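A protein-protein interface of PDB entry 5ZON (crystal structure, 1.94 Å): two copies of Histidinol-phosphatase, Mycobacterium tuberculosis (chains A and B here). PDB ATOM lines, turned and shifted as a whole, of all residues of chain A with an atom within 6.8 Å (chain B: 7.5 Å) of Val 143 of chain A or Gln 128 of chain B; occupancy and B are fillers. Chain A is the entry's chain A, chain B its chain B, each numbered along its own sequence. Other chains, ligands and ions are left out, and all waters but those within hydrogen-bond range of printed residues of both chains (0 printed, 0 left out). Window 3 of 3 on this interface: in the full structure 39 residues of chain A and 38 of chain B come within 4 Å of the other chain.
The side-chain amide oxygen (OE1) of Gln 128 of chain A sits at hydrogen-bond distance from the guanidinium group (NH1) of Arg 129 of chain B (3.2 Å). OE1 of Gln 128 of chain B lies within hydrogen-bond range of NH1 of Arg 129 of chain A. NH2 of Arg 129 of chain A is in hydrogen-bond range of O of Ala 126 of chain B (2.8 Å). NH2 of Arg 129 of chain B is in hydrogen-bond range of O of Ala 126 of chain A (2.9 Å). OE1 of Gln 128 of chain A lies close to OE1 of Gln 128 of chain B (3.5 Å).
The backbone carbonyl oxygen of Leu 127 of chain B lies within hydrogen-bond range of the guanidinium group of Arg 129 of chain B (2.9 Å). O of Ala 126 of chain A sits at hydrogen-bond distance from NE2 of Gln 128 of chain A, 3.2 Å away. N of Ala 124 of chain B is in hydrogen-bond range of O of Arg 129 of chain B, at 2.9 Å. O of Gln 128 of chain B lies within hydrogen-bond range of N of Asp 144 of chain B, at 2.7 Å. O of Ala 126 of chain B lies within hydrogen-bond range of NE2 of Gln 128 of chain B (3.2 Å). NH1 of Arg 129 of chain A is in hydrogen-bond range of O of Leu 127 of chain A (2.9 Å).
Among the printed residues, pairs that only touch across the chains: Leu 127 of chain A with Gln 128 of chain B, Gln 128 of chain A with Leu 127 of chain B, Arg 129 of chain A with Pro 103 of chain B and Val 143 of chain A with Gln 128 of chain B.
Gln 128 of chain B touches four residues of chain A. No residue of chain B comes within 4 Å of Asp 144 of chain A. Of the printed residues of chain A, Ala 126 of chain B touches Arg 129. Printed residues of chain A within 4 Å of Leu 127 of chain B: Gln 128. Of the printed residues of chain A, Arg 129 of chain B touches Ala 126 and Gln 128. Ser 142 of chain B touches none of the printed residues of chain A. Ala 124 of chain B touches none of the printed residues of chain A. The nearest printed residue of chain A that does not touch Arg 129 of chain B is Leu 127 of chain A (4.8 Å).
Printed residues of chain B that touch a printed residue of chain A: Pro 103, Ala 126, Leu 127, Gln 128 and Arg 129. Hydrophobic or aromatic side chains of chain B that line the printed part of chain A: Pro 103. Of the 15 printed residues of chain A, 5 touch a printed residue of chain B. Hydrophobic or aromatic side chains of chain A that line the printed part of chain B: Val 143. Among the printed residues, 9 pairs touch across the chains. Among the printed residues, no Asp or Glu carboxylate lies within 4 Å of a Lys or Arg side-chain nitrogen of the other chain.
Ala 126 of chain A touches Arg 129 of chain B, and with the chains exchanged Arg 129 of chain A touches Ala 126 of chain B. Leu 127 of chain A touches Gln 128 of chain B, and with the chains exchanged Gln 128 of chain A touches Leu 127 of chain B. Gln 128 of chain A touches its own counterpart, Gln 128 of chain B. Gln 128 of chain A touches Arg 129 of chain B, and with the chains exchanged Arg 129 of chain A touches Gln 128 of chain B. 8 positions are printed for both chains. Of the 9 pairs that touch across the chains among the printed residues, 7 have their exchanged pair printed and touching as well.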
ATOM      1  N   ALA A 126       9.371  -5.073 -20.657  1.00  0.00           N
ATOM      2  CA  ALA A 126      10.299  -5.604 -19.649  1.00  0.00           C
ATOM      3  C   ALA A 126      10.829  -4.504 -18.718  1.00  0.00           C
ATOM      4  O   ALA A 126      11.489  -4.814 -17.726  1.00  0.00           O
ATOM      5  CB  ALA A 126      11.438  -6.389 -20.264  1.00  0.00           C
ATOM      6  N   LEU A 127      10.574  -3.231 -19.019  1.00  0.00           N
ATOM      7  CA  LEU A 127      10.843  -2.128 -18.082  1.00  0.00           C
ATOM      8  C   LEU A 127       9.532  -1.782 -17.370  1.00  0.00           C
ATOM      9  O   LEU A 127       9.488  -0.824 -16.597  1.00  0.00           O
ATOM     10  CB  LEU A 127      11.347  -0.893 -18.844  1.00  0.00           C
ATOM     11  CG  LEU A 127      12.685  -1.056 -19.588  1.00  0.00           C
ATOM     12  CD1 LEU A 127      13.116   0.248 -20.266  1.00  0.00           C
ATOM     13  CD2 LEU A 127      13.767  -1.568 -18.651  1.00  0.00           C
ATOM     14  N   GLN A 128       8.464  -2.509 -17.703  1.00  0.00           N
ATOM     15  CA  GLN A 128       7.114  -2.216 -17.211  1.00  0.00           C
ATOM     16  C   GLN A 128       6.747  -0.740 -17.501  1.00  0.00           C
ATOM     17  O   GLN A 128       6.185  -0.031 -16.634  1.00  0.00           O
ATOM     18  CB  GLN A 128       7.003  -2.556 -15.711  1.00  0.00           C
ATOM     19  CG  GLN A 128       7.285  -4.017 -15.350  1.00  0.00           C
ATOM     20  CD  GLN A 128       8.733  -4.490 -15.385  1.00  0.00           C
ATOM     21  OE1 GLN A 128       9.664  -3.854 -14.879  1.00  0.00           O
ATOM     22  NE2 GLN A 128       8.951  -5.658 -15.979  1.00  0.00           N
ATOM     23  N   ARG A 129       7.029  -0.246 -18.705  1.00  0.00           N
ATOM     24  CA  ARG A 129       6.866   1.214 -18.977  1.00  0.00           C
ATOM     25  C   ARG A 129       6.300   1.433 -20.381  1.00  0.00           C
ATOM     26  O   ARG A 129       6.602   0.698 -21.310  1.00  0.00           O
ATOM     27  CB  ARG A 129       8.213   1.955 -18.844  1.00  0.00           C
ATOM     28  CG  ARG A 129       8.510   2.354 -17.405  1.00  0.00           C
ATOM     29  CD  ARG A 129       9.927   2.755 -17.130  1.00  0.00           C
ATOM     30  NE  ARG A 129      10.024   3.378 -15.817  1.00  0.00           N
ATOM     31  CZ  ARG A 129      10.210   2.684 -14.701  1.00  0.00           C
ATOM     32  NH1 ARG A 129      10.114   1.364 -14.721  1.00  0.00           N
ATOM     33  NH2 ARG A 129      10.516   3.300 -13.567  1.00  0.00           N
ATOM     34  N   ARG A 130       5.526   2.494 -20.530  1.00  0.00           N
ATOM     35  CA  ARG A 130       5.025   2.923 -21.832  1.00  0.00           C
ATOM     36  C   ARG A 130       5.045   4.457 -21.827  1.00  0.00           C
ATOM     37  O   ARG A 130       4.759   5.074 -20.783  1.00  0.00           O
ATOM     38  CB  ARG A 130       3.611   2.377 -22.086  1.00  0.00           C
ATOM     39  CG  ARG A 130       3.085   2.707 -23.481  1.00  0.00           C
ATOM     40  CD  ARG A 130       1.736   2.077 -23.793  1.00  0.00           C
ATOM     41  NE  ARG A 130       1.822   0.627 -23.822  1.00  0.00           N
ATOM     42  CZ  ARG A 130       0.797  -0.171 -24.114  1.00  0.00           C
ATOM     43  NH1 ARG A 130      -0.431   0.325 -24.198  1.00  0.00           N
ATOM     44  NH2 ARG A 130       1.021  -1.452 -24.347  1.00  0.00           N
ATOM     45  N   ALA A 141       3.395   9.057 -19.515  1.00  0.00           N
ATOM     46  CA  ALA A 141       4.073   7.802 -19.254  1.00  0.00           C
ATOM     47  C   ALA A 141       3.272   7.013 -18.210  1.00  0.00           C
ATOM     48  O   ALA A 141       2.544   7.596 -17.403  1.00  0.00           O
ATOM     49  CB  ALA A 141       5.471   8.068 -18.770  1.00  0.00           C
ATOM     50  N   SER A 142       3.383   5.695 -18.258  1.00  0.00           N
ATOM     51  CA  SER A 142       2.866   4.875 -17.186  1.00  0.00           C
ATOM     52  C   SER A 142       3.937   3.861 -16.779  1.00  0.00           C
ATOM     53  O   SER A 142       4.673   3.343 -17.636  1.00  0.00           O
ATOM     54  CB  SER A 142       1.619   4.153 -17.619  1.00  0.00           C
ATOM     55  OG  SER A 142       1.891   3.425 -18.805  1.00  0.00           O
ATOM     56  N   VAL A 143       4.000   3.594 -15.476  1.00  0.00           N
ATOM     57  CA  VAL A 143       4.889   2.601 -14.912  1.00  0.00           C
ATOM     58  C   VAL A 143       4.014   1.506 -14.294  1.00  0.00           C
ATOM     59  O   VAL A 143       3.144   1.817 -13.454  1.00  0.00           O
ATOM     60  CB  VAL A 143       5.834   3.206 -13.854  1.00  0.00           C
ATOM     61  CG1 VAL A 143       6.883   2.192 -13.395  1.00  0.00           C
ATOM     62  CG2 VAL A 143       6.495   4.485 -14.350  1.00  0.00           C
ATOM     63  N   ASP A 144       4.244   0.265 -14.728  1.00  0.00           N
ATOM     64  CA  ASP A 144       3.477  -0.927 -14.348  1.00  0.00           C
ATOM     65  C   ASP A 144       1.982  -0.625 -14.382  1.00  0.00           C
ATOM     66  O   ASP A 144       1.293  -0.863 -13.406  1.00  0.00           O
ATOM     67  CB  ASP A 144       3.880  -1.512 -12.991  1.00  0.00           C
ATOM     68  CG  ASP A 144       4.697  -0.597 -12.100  1.00  0.00           C
ATOM     69  N   GLY A 145       1.511  -0.059 -15.480  1.00  0.00           N
ATOM     70  CA  GLY A 145       0.096   0.238 -15.656  1.00  0.00           C
ATOM     71  C   GLY A 145      -0.555   0.922 -14.457  1.00  0.00           C
ATOM     72  O   GLY A 145      -1.733   0.712 -14.230  1.00  0.00           O
ATOM     73  N   ALA A 146       0.173   1.729 -13.682  1.00  0.00           N
ATOM     74  CA  ALA A 146      -0.468   2.706 -12.794  1.00  0.00           C
ATOM     75  C   ALA A 146      -1.095   3.795 -13.669  1.00  0.00           C
ATOM     76  O   ALA A 146      -1.042   3.680 -14.891  1.00  0.00           O
ATOM     77  CB  ALA A 146       0.515   3.251 -11.781  1.00  0.00           C
ATOM     78  N   ARG A 147      -1.764   4.788 -13.078  1.00  0.00           N
ATOM     79  CA  ARG A 147      -2.350   5.881 -13.853  1.00  0.00           C
ATOM     80  C   ARG A 147      -1.241   6.605 -14.627  1.00  0.00           C
ATOM     81  O   ARG A 147      -0.152   6.766 -14.105  1.00  0.00           O
ATOM     82  CB  ARG A 147      -3.055   6.866 -12.911  1.00  0.00           C
ATOM     83  CG  ARG A 147      -4.498   6.484 -12.586  1.00  0.00           C
ATOM     84  CD  ARG A 147      -4.955   6.553 -11.130  1.00  0.00           C
ATOM     85  N   PRO A 148      -1.537   7.064 -15.853  1.00  0.00           N
ATOM     86  CA  PRO A 148      -0.600   7.895 -16.631  1.00  0.00           C
ATOM     87  C   PRO A 148      -0.229   9.185 -15.883  1.00  0.00           C
ATOM     88  O   PRO A 148      -1.062   9.725 -15.138  1.00  0.00           O
ATOM     89  CB  PRO A 148      -1.401   8.277 -17.883  1.00  0.00           C
ATOM     90  CG  PRO A 148      -2.406   7.156 -18.048  1.00  0.00           C
ATOM     91  CD  PRO A 148      -2.759   6.766 -16.628  1.00  0.00           C
ATOM     92  N   HIS A 149       1.001   9.651 -16.062  1.00  0.00           N
ATOM     93  CA  HIS A 149       1.404  11.004 -15.650  1.00  0.00           C
ATOM     94  C   HIS A 149       1.826  11.814 -16.882  1.00  0.00           C
ATOM     95  O   HIS A 149       2.469  11.295 -17.786  1.00  0.00           O
ATOM     96  CB  HIS A 149       2.443  11.026 -14.513  1.00  0.00           C
ATOM     97  CG  HIS A 149       3.340   9.839 -14.443  1.00  0.00           C
ATOM     98  ND1 HIS A 149       4.588   9.835 -15.043  1.00  0.00           N
ATOM     99  CD2 HIS A 149       3.204   8.637 -13.832  1.00  0.00           C
ATOM    100  CE1 HIS A 149       5.178   8.670 -14.813  1.00  0.00           C
ATOM    101  NE2 HIS A 149       4.340   7.911 -14.084  1.00  0.00           N
ATOM    102  N   GLU A 205      10.583  13.002 -20.063  1.00  0.00           N
ATOM    103  CA  GLU A 205      10.155  12.984 -18.655  1.00  0.00           C
ATOM    104  C   GLU A 205      10.820  14.119 -17.875  1.00  0.00           C
ATOM    105  O   GLU A 205      10.415  14.376 -16.758  1.00  0.00           O
ATOM    106  CB  GLU A 205      10.581  11.692 -17.948  1.00  0.00           C
ATOM    107  CG  GLU A 205       9.862  10.443 -18.417  1.00  0.00           C
ATOM    108  CD  GLU A 205      10.274   9.214 -17.614  1.00  0.00           C
ATOM    109  OE1 GLU A 205      10.377   8.114 -18.214  1.00  0.00           O
ATOM    110  OE2 GLU A 205      10.597   9.386 -16.393  1.00  0.00           O
ATOM    111  N   ARG B  28      10.474   4.379  -1.834  1.00  0.00           N
ATOM    112  CA  ARG B  28       9.400   4.527  -2.837  1.00  0.00           C
ATOM    113  C   ARG B  28       8.601   5.809  -2.580  1.00  0.00           C
ATOM    114  O   ARG B  28       8.293   6.574  -3.525  1.00  0.00           O
ATOM    115  CB  ARG B  28       8.377   3.389  -2.742  1.00  0.00           C
ATOM    116  CG  ARG B  28       8.767   2.150  -3.518  1.00  0.00           C
ATOM    117  CD  ARG B  28       7.553   1.271  -3.786  1.00  0.00           C
ATOM    118  NE  ARG B  28       7.263   0.338  -2.717  1.00  0.00           N
ATOM    119  CZ  ARG B  28       7.776  -0.889  -2.630  1.00  0.00           C
ATOM    120  NH1 ARG B  28       7.510  -1.647  -1.580  1.00  0.00           N
ATOM    121  NH2 ARG B  28       8.559  -1.346  -3.593  1.00  0.00           N
ATOM    122  N   PRO B 103      15.094   6.197 -12.613  1.00  0.00           N
ATOM    123  CA  PRO B 103      14.753   5.163 -11.605  1.00  0.00           C
ATOM    124  C   PRO B 103      15.903   4.172 -11.323  1.00  0.00           C
ATOM    125  O   PRO B 103      15.694   3.211 -10.573  1.00  0.00           O
ATOM    126  CB  PRO B 103      13.587   4.392 -12.254  1.00  0.00           C
ATOM    127  CG  PRO B 103      13.882   4.496 -13.756  1.00  0.00           C
ATOM    128  CD  PRO B 103      14.467   5.885 -13.916  1.00  0.00           C
ATOM    129  N   SER B 123      18.333  -3.554  -3.856  1.00  0.00           N
ATOM    130  CA  SER B 123      16.903  -3.406  -3.987  1.00  0.00           C
ATOM    131  C   SER B 123      16.582  -2.110  -4.737  1.00  0.00           C
ATOM    132  O   SER B 123      16.831  -1.021  -4.201  1.00  0.00           O
ATOM    133  CB  SER B 123      16.250  -3.427  -2.618  1.00  0.00           C
ATOM    134  OG  SER B 123      14.845  -3.576  -2.763  1.00  0.00           O
ATOM    135  N   ALA B 124      16.006  -2.259  -5.939  1.00  0.00           N
ATOM    136  CA  ALA B 124      15.721  -1.143  -6.858  1.00  0.00           C
ATOM    137  C   ALA B 124      14.207  -1.072  -7.132  1.00  0.00           C
ATOM    138  O   ALA B 124      13.739  -1.553  -8.166  1.00  0.00           O
ATOM    139  CB  ALA B 124      16.516  -1.296  -8.157  1.00  0.00           C
ATOM    140  N   PRO B 125      13.449  -0.459  -6.207  1.00  0.00           N
ATOM    141  CA  PRO B 125      11.992  -0.494  -6.264  1.00  0.00           C
ATOM    142  C   PRO B 125      11.411   0.204  -7.496  1.00  0.00           C
ATOM    143  O   PRO B 125      10.399  -0.254  -8.005  1.00  0.00           O
ATOM    144  CB  PRO B 125      11.452   0.120  -4.974  1.00  0.00           C
ATOM    145  CG  PRO B 125      12.627   0.761  -4.309  1.00  0.00           C
ATOM    146  CD  PRO B 125      13.855   0.127  -4.919  1.00  0.00           C
ATOM    147  N   ALA B 126      12.074   1.233  -8.025  1.00  0.00           N
ATOM    148  CA  ALA B 126      11.539   1.924  -9.222  1.00  0.00           C
ATOM    149  C   ALA B 126      11.921   1.180 -10.508  1.00  0.00           C
ATOM    150  O   ALA B 126      11.426   1.549 -11.564  1.00  0.00           O
ATOM    151  CB  ALA B 126      11.989   3.362  -9.229  1.00  0.00           C
ATOM    152  N   LEU B 127      12.808   0.183 -10.444  1.00  0.00           N
ATOM    153  CA  LEU B 127      13.058  -0.717 -11.581  1.00  0.00           C
ATOM    154  C   LEU B 127      12.229  -1.986 -11.381  1.00  0.00           C
ATOM    155  O   LEU B 127      12.348  -2.933 -12.167  1.00  0.00           O
ATOM    156  CB  LEU B 127      14.551  -1.085 -11.641  1.00  0.00           C
ATOM    157  CG  LEU B 127      15.538   0.056 -11.887  1.00  0.00           C
ATOM    158  CD1 LEU B 127      16.962  -0.489 -12.023  1.00  0.00           C
ATOM    159  CD2 LEU B 127      15.161   0.860 -13.126  1.00  0.00           C
ATOM    160  N   GLN B 128      11.485  -2.042 -10.288  1.00  0.00           N
ATOM    161  CA  GLN B 128      10.739  -3.242  -9.882  1.00  0.00           C
ATOM    162  C   GLN B 128      11.693  -4.459  -9.812  1.00  0.00           C
ATOM    163  O   GLN B 128      11.345  -5.573 -10.250  1.00  0.00           O
ATOM    164  CB  GLN B 128       9.543  -3.491 -10.817  1.00  0.00           C
ATOM    165  CG  GLN B 128       8.521  -2.350 -10.908  1.00  0.00           C
ATOM    166  CD  GLN B 128       8.914  -1.089 -11.668  1.00  0.00           C
ATOM    167  OE1 GLN B 128       9.451  -1.111 -12.786  1.00  0.00           O
ATOM    168  NE2 GLN B 128       8.636   0.062 -11.063  1.00  0.00           N
ATOM    169  N   ARG B 129      12.893  -4.293  -9.247  1.00  0.00           N
ATOM    170  CA  ARG B 129      13.895  -5.382  -9.304  1.00  0.00           C
ATOM    171  C   ARG B 129      14.630  -5.515  -7.964  1.00  0.00           C
ATOM    172  O   ARG B 129      14.853  -4.521  -7.268  1.00  0.00           O
ATOM    173  CB  ARG B 129      14.906  -5.128 -10.434  1.00  0.00           C
ATOM    174  CG  ARG B 129      14.411  -5.629 -11.784  1.00  0.00           C
ATOM    175  CD  ARG B 129      15.156  -5.109 -12.993  1.00  0.00           C
ATOM    176  NE  ARG B 129      14.732  -5.869 -14.164  1.00  0.00           N
ATOM    177  CZ  ARG B 129      13.652  -5.595 -14.885  1.00  0.00           C
ATOM    178  NH1 ARG B 129      12.764  -4.711 -14.456  1.00  0.00           N
ATOM    179  NH2 ARG B 129      13.440  -6.223 -16.020  1.00  0.00           N
ATOM    180  N   ARG B 130      15.008  -6.750  -7.633  1.00  0.00           N
ATOM    181  CA  ARG B 130      15.875  -6.988  -6.473  1.00  0.00           C
ATOM    182  C   ARG B 130      16.877  -8.084  -6.856  1.00  0.00           C
ATOM    183  O   ARG B 130      16.517  -9.012  -7.599  1.00  0.00           O
ATOM    184  CB  ARG B 130      15.028  -7.375  -5.255  1.00  0.00           C
ATOM    185  CG  ARG B 130      15.844  -7.571  -3.979  1.00  0.00           C
ATOM    186  CD  ARG B 130      14.985  -7.888  -2.779  1.00  0.00           C
ATOM    187  NE  ARG B 130      14.170  -6.759  -2.390  1.00  0.00           N
ATOM    188  CZ  ARG B 130      13.312  -6.767  -1.366  1.00  0.00           C
ATOM    189  NH1 ARG B 130      13.086  -7.887  -0.696  1.00  0.00           N
ATOM    190  NH2 ARG B 130      12.713  -5.643  -1.005  1.00  0.00           N
ATOM    191  N   TRP B 131      18.117  -7.937  -6.411  1.00  0.00           N
ATOM    192  CA  TRP B 131      19.135  -8.979  -6.563  1.00  0.00           C
ATOM    193  C   TRP B 131      19.666  -9.335  -5.169  1.00  0.00           C
ATOM    194  O   TRP B 131      19.773  -8.462  -4.296  1.00  0.00           O
ATOM    195  CB  TRP B 131      20.296  -8.521  -7.455  1.00  0.00           C
ATOM    196  CG  TRP B 131      19.917  -8.085  -8.840  1.00  0.00           C
ATOM    197  CD1 TRP B 131      20.086  -8.783  -9.998  1.00  0.00           C
ATOM    198  CD2 TRP B 131      19.409  -6.796  -9.219  1.00  0.00           C
ATOM    199  NE1 TRP B 131      19.679  -8.033 -11.076  1.00  0.00           N
ATOM    200  CE2 TRP B 131      19.258  -6.808 -10.623  1.00  0.00           C
ATOM    201  CE3 TRP B 131      19.043  -5.650  -8.502  1.00  0.00           C
ATOM    202  CZ2 TRP B 131      18.775  -5.702 -11.325  1.00  0.00           C
ATOM    203  CZ3 TRP B 131      18.566  -4.563  -9.202  1.00  0.00           C
ATOM    204  CH2 TRP B 131      18.443  -4.586 -10.591  1.00  0.00           C
ATOM    205  N   SER B 142      14.749 -11.060  -8.771  1.00  0.00           N
ATOM    206  CA  SER B 142      13.342 -11.070  -9.014  1.00  0.00           C
ATOM    207  C   SER B 142      12.947  -9.811  -9.791  1.00  0.00           C
ATOM    208  O   SER B 142      13.476  -8.713  -9.501  1.00  0.00           O
ATOM    209  CB  SER B 142      12.624 -11.080  -7.686  1.00  0.00           C
ATOM    210  OG  SER B 142      11.220 -11.146  -7.882  1.00  0.00           O
ATOM    211  N   VAL B 143      11.966  -9.962 -10.678  1.00  0.00           N
ATOM    212  CA  VAL B 143      11.371  -8.825 -11.382  1.00  0.00           C
ATOM    213  C   VAL B 143       9.899  -8.739 -10.967  1.00  0.00           C
ATOM    214  O   VAL B 143       9.160  -9.721 -11.142  1.00  0.00           O
ATOM    215  CB  VAL B 143      11.507  -8.957 -12.914  1.00  0.00           C
ATOM    216  CG2 VAL B 143      12.919  -9.339 -13.336  1.00  0.00           C
ATOM    217  N   ASP B 144       9.506  -7.587 -10.411  1.00  0.00           N
ATOM    218  CA  ASP B 144       8.174  -7.353  -9.809  1.00  0.00           C
ATOM    219  C   ASP B 144       7.688  -8.574  -9.012  1.00  0.00           C
ATOM    220  O   ASP B 144       8.028  -8.774  -7.831  1.00  0.00           O
ATOM    221  CB  ASP B 144       7.130  -6.976 -10.863  1.00  0.00           C
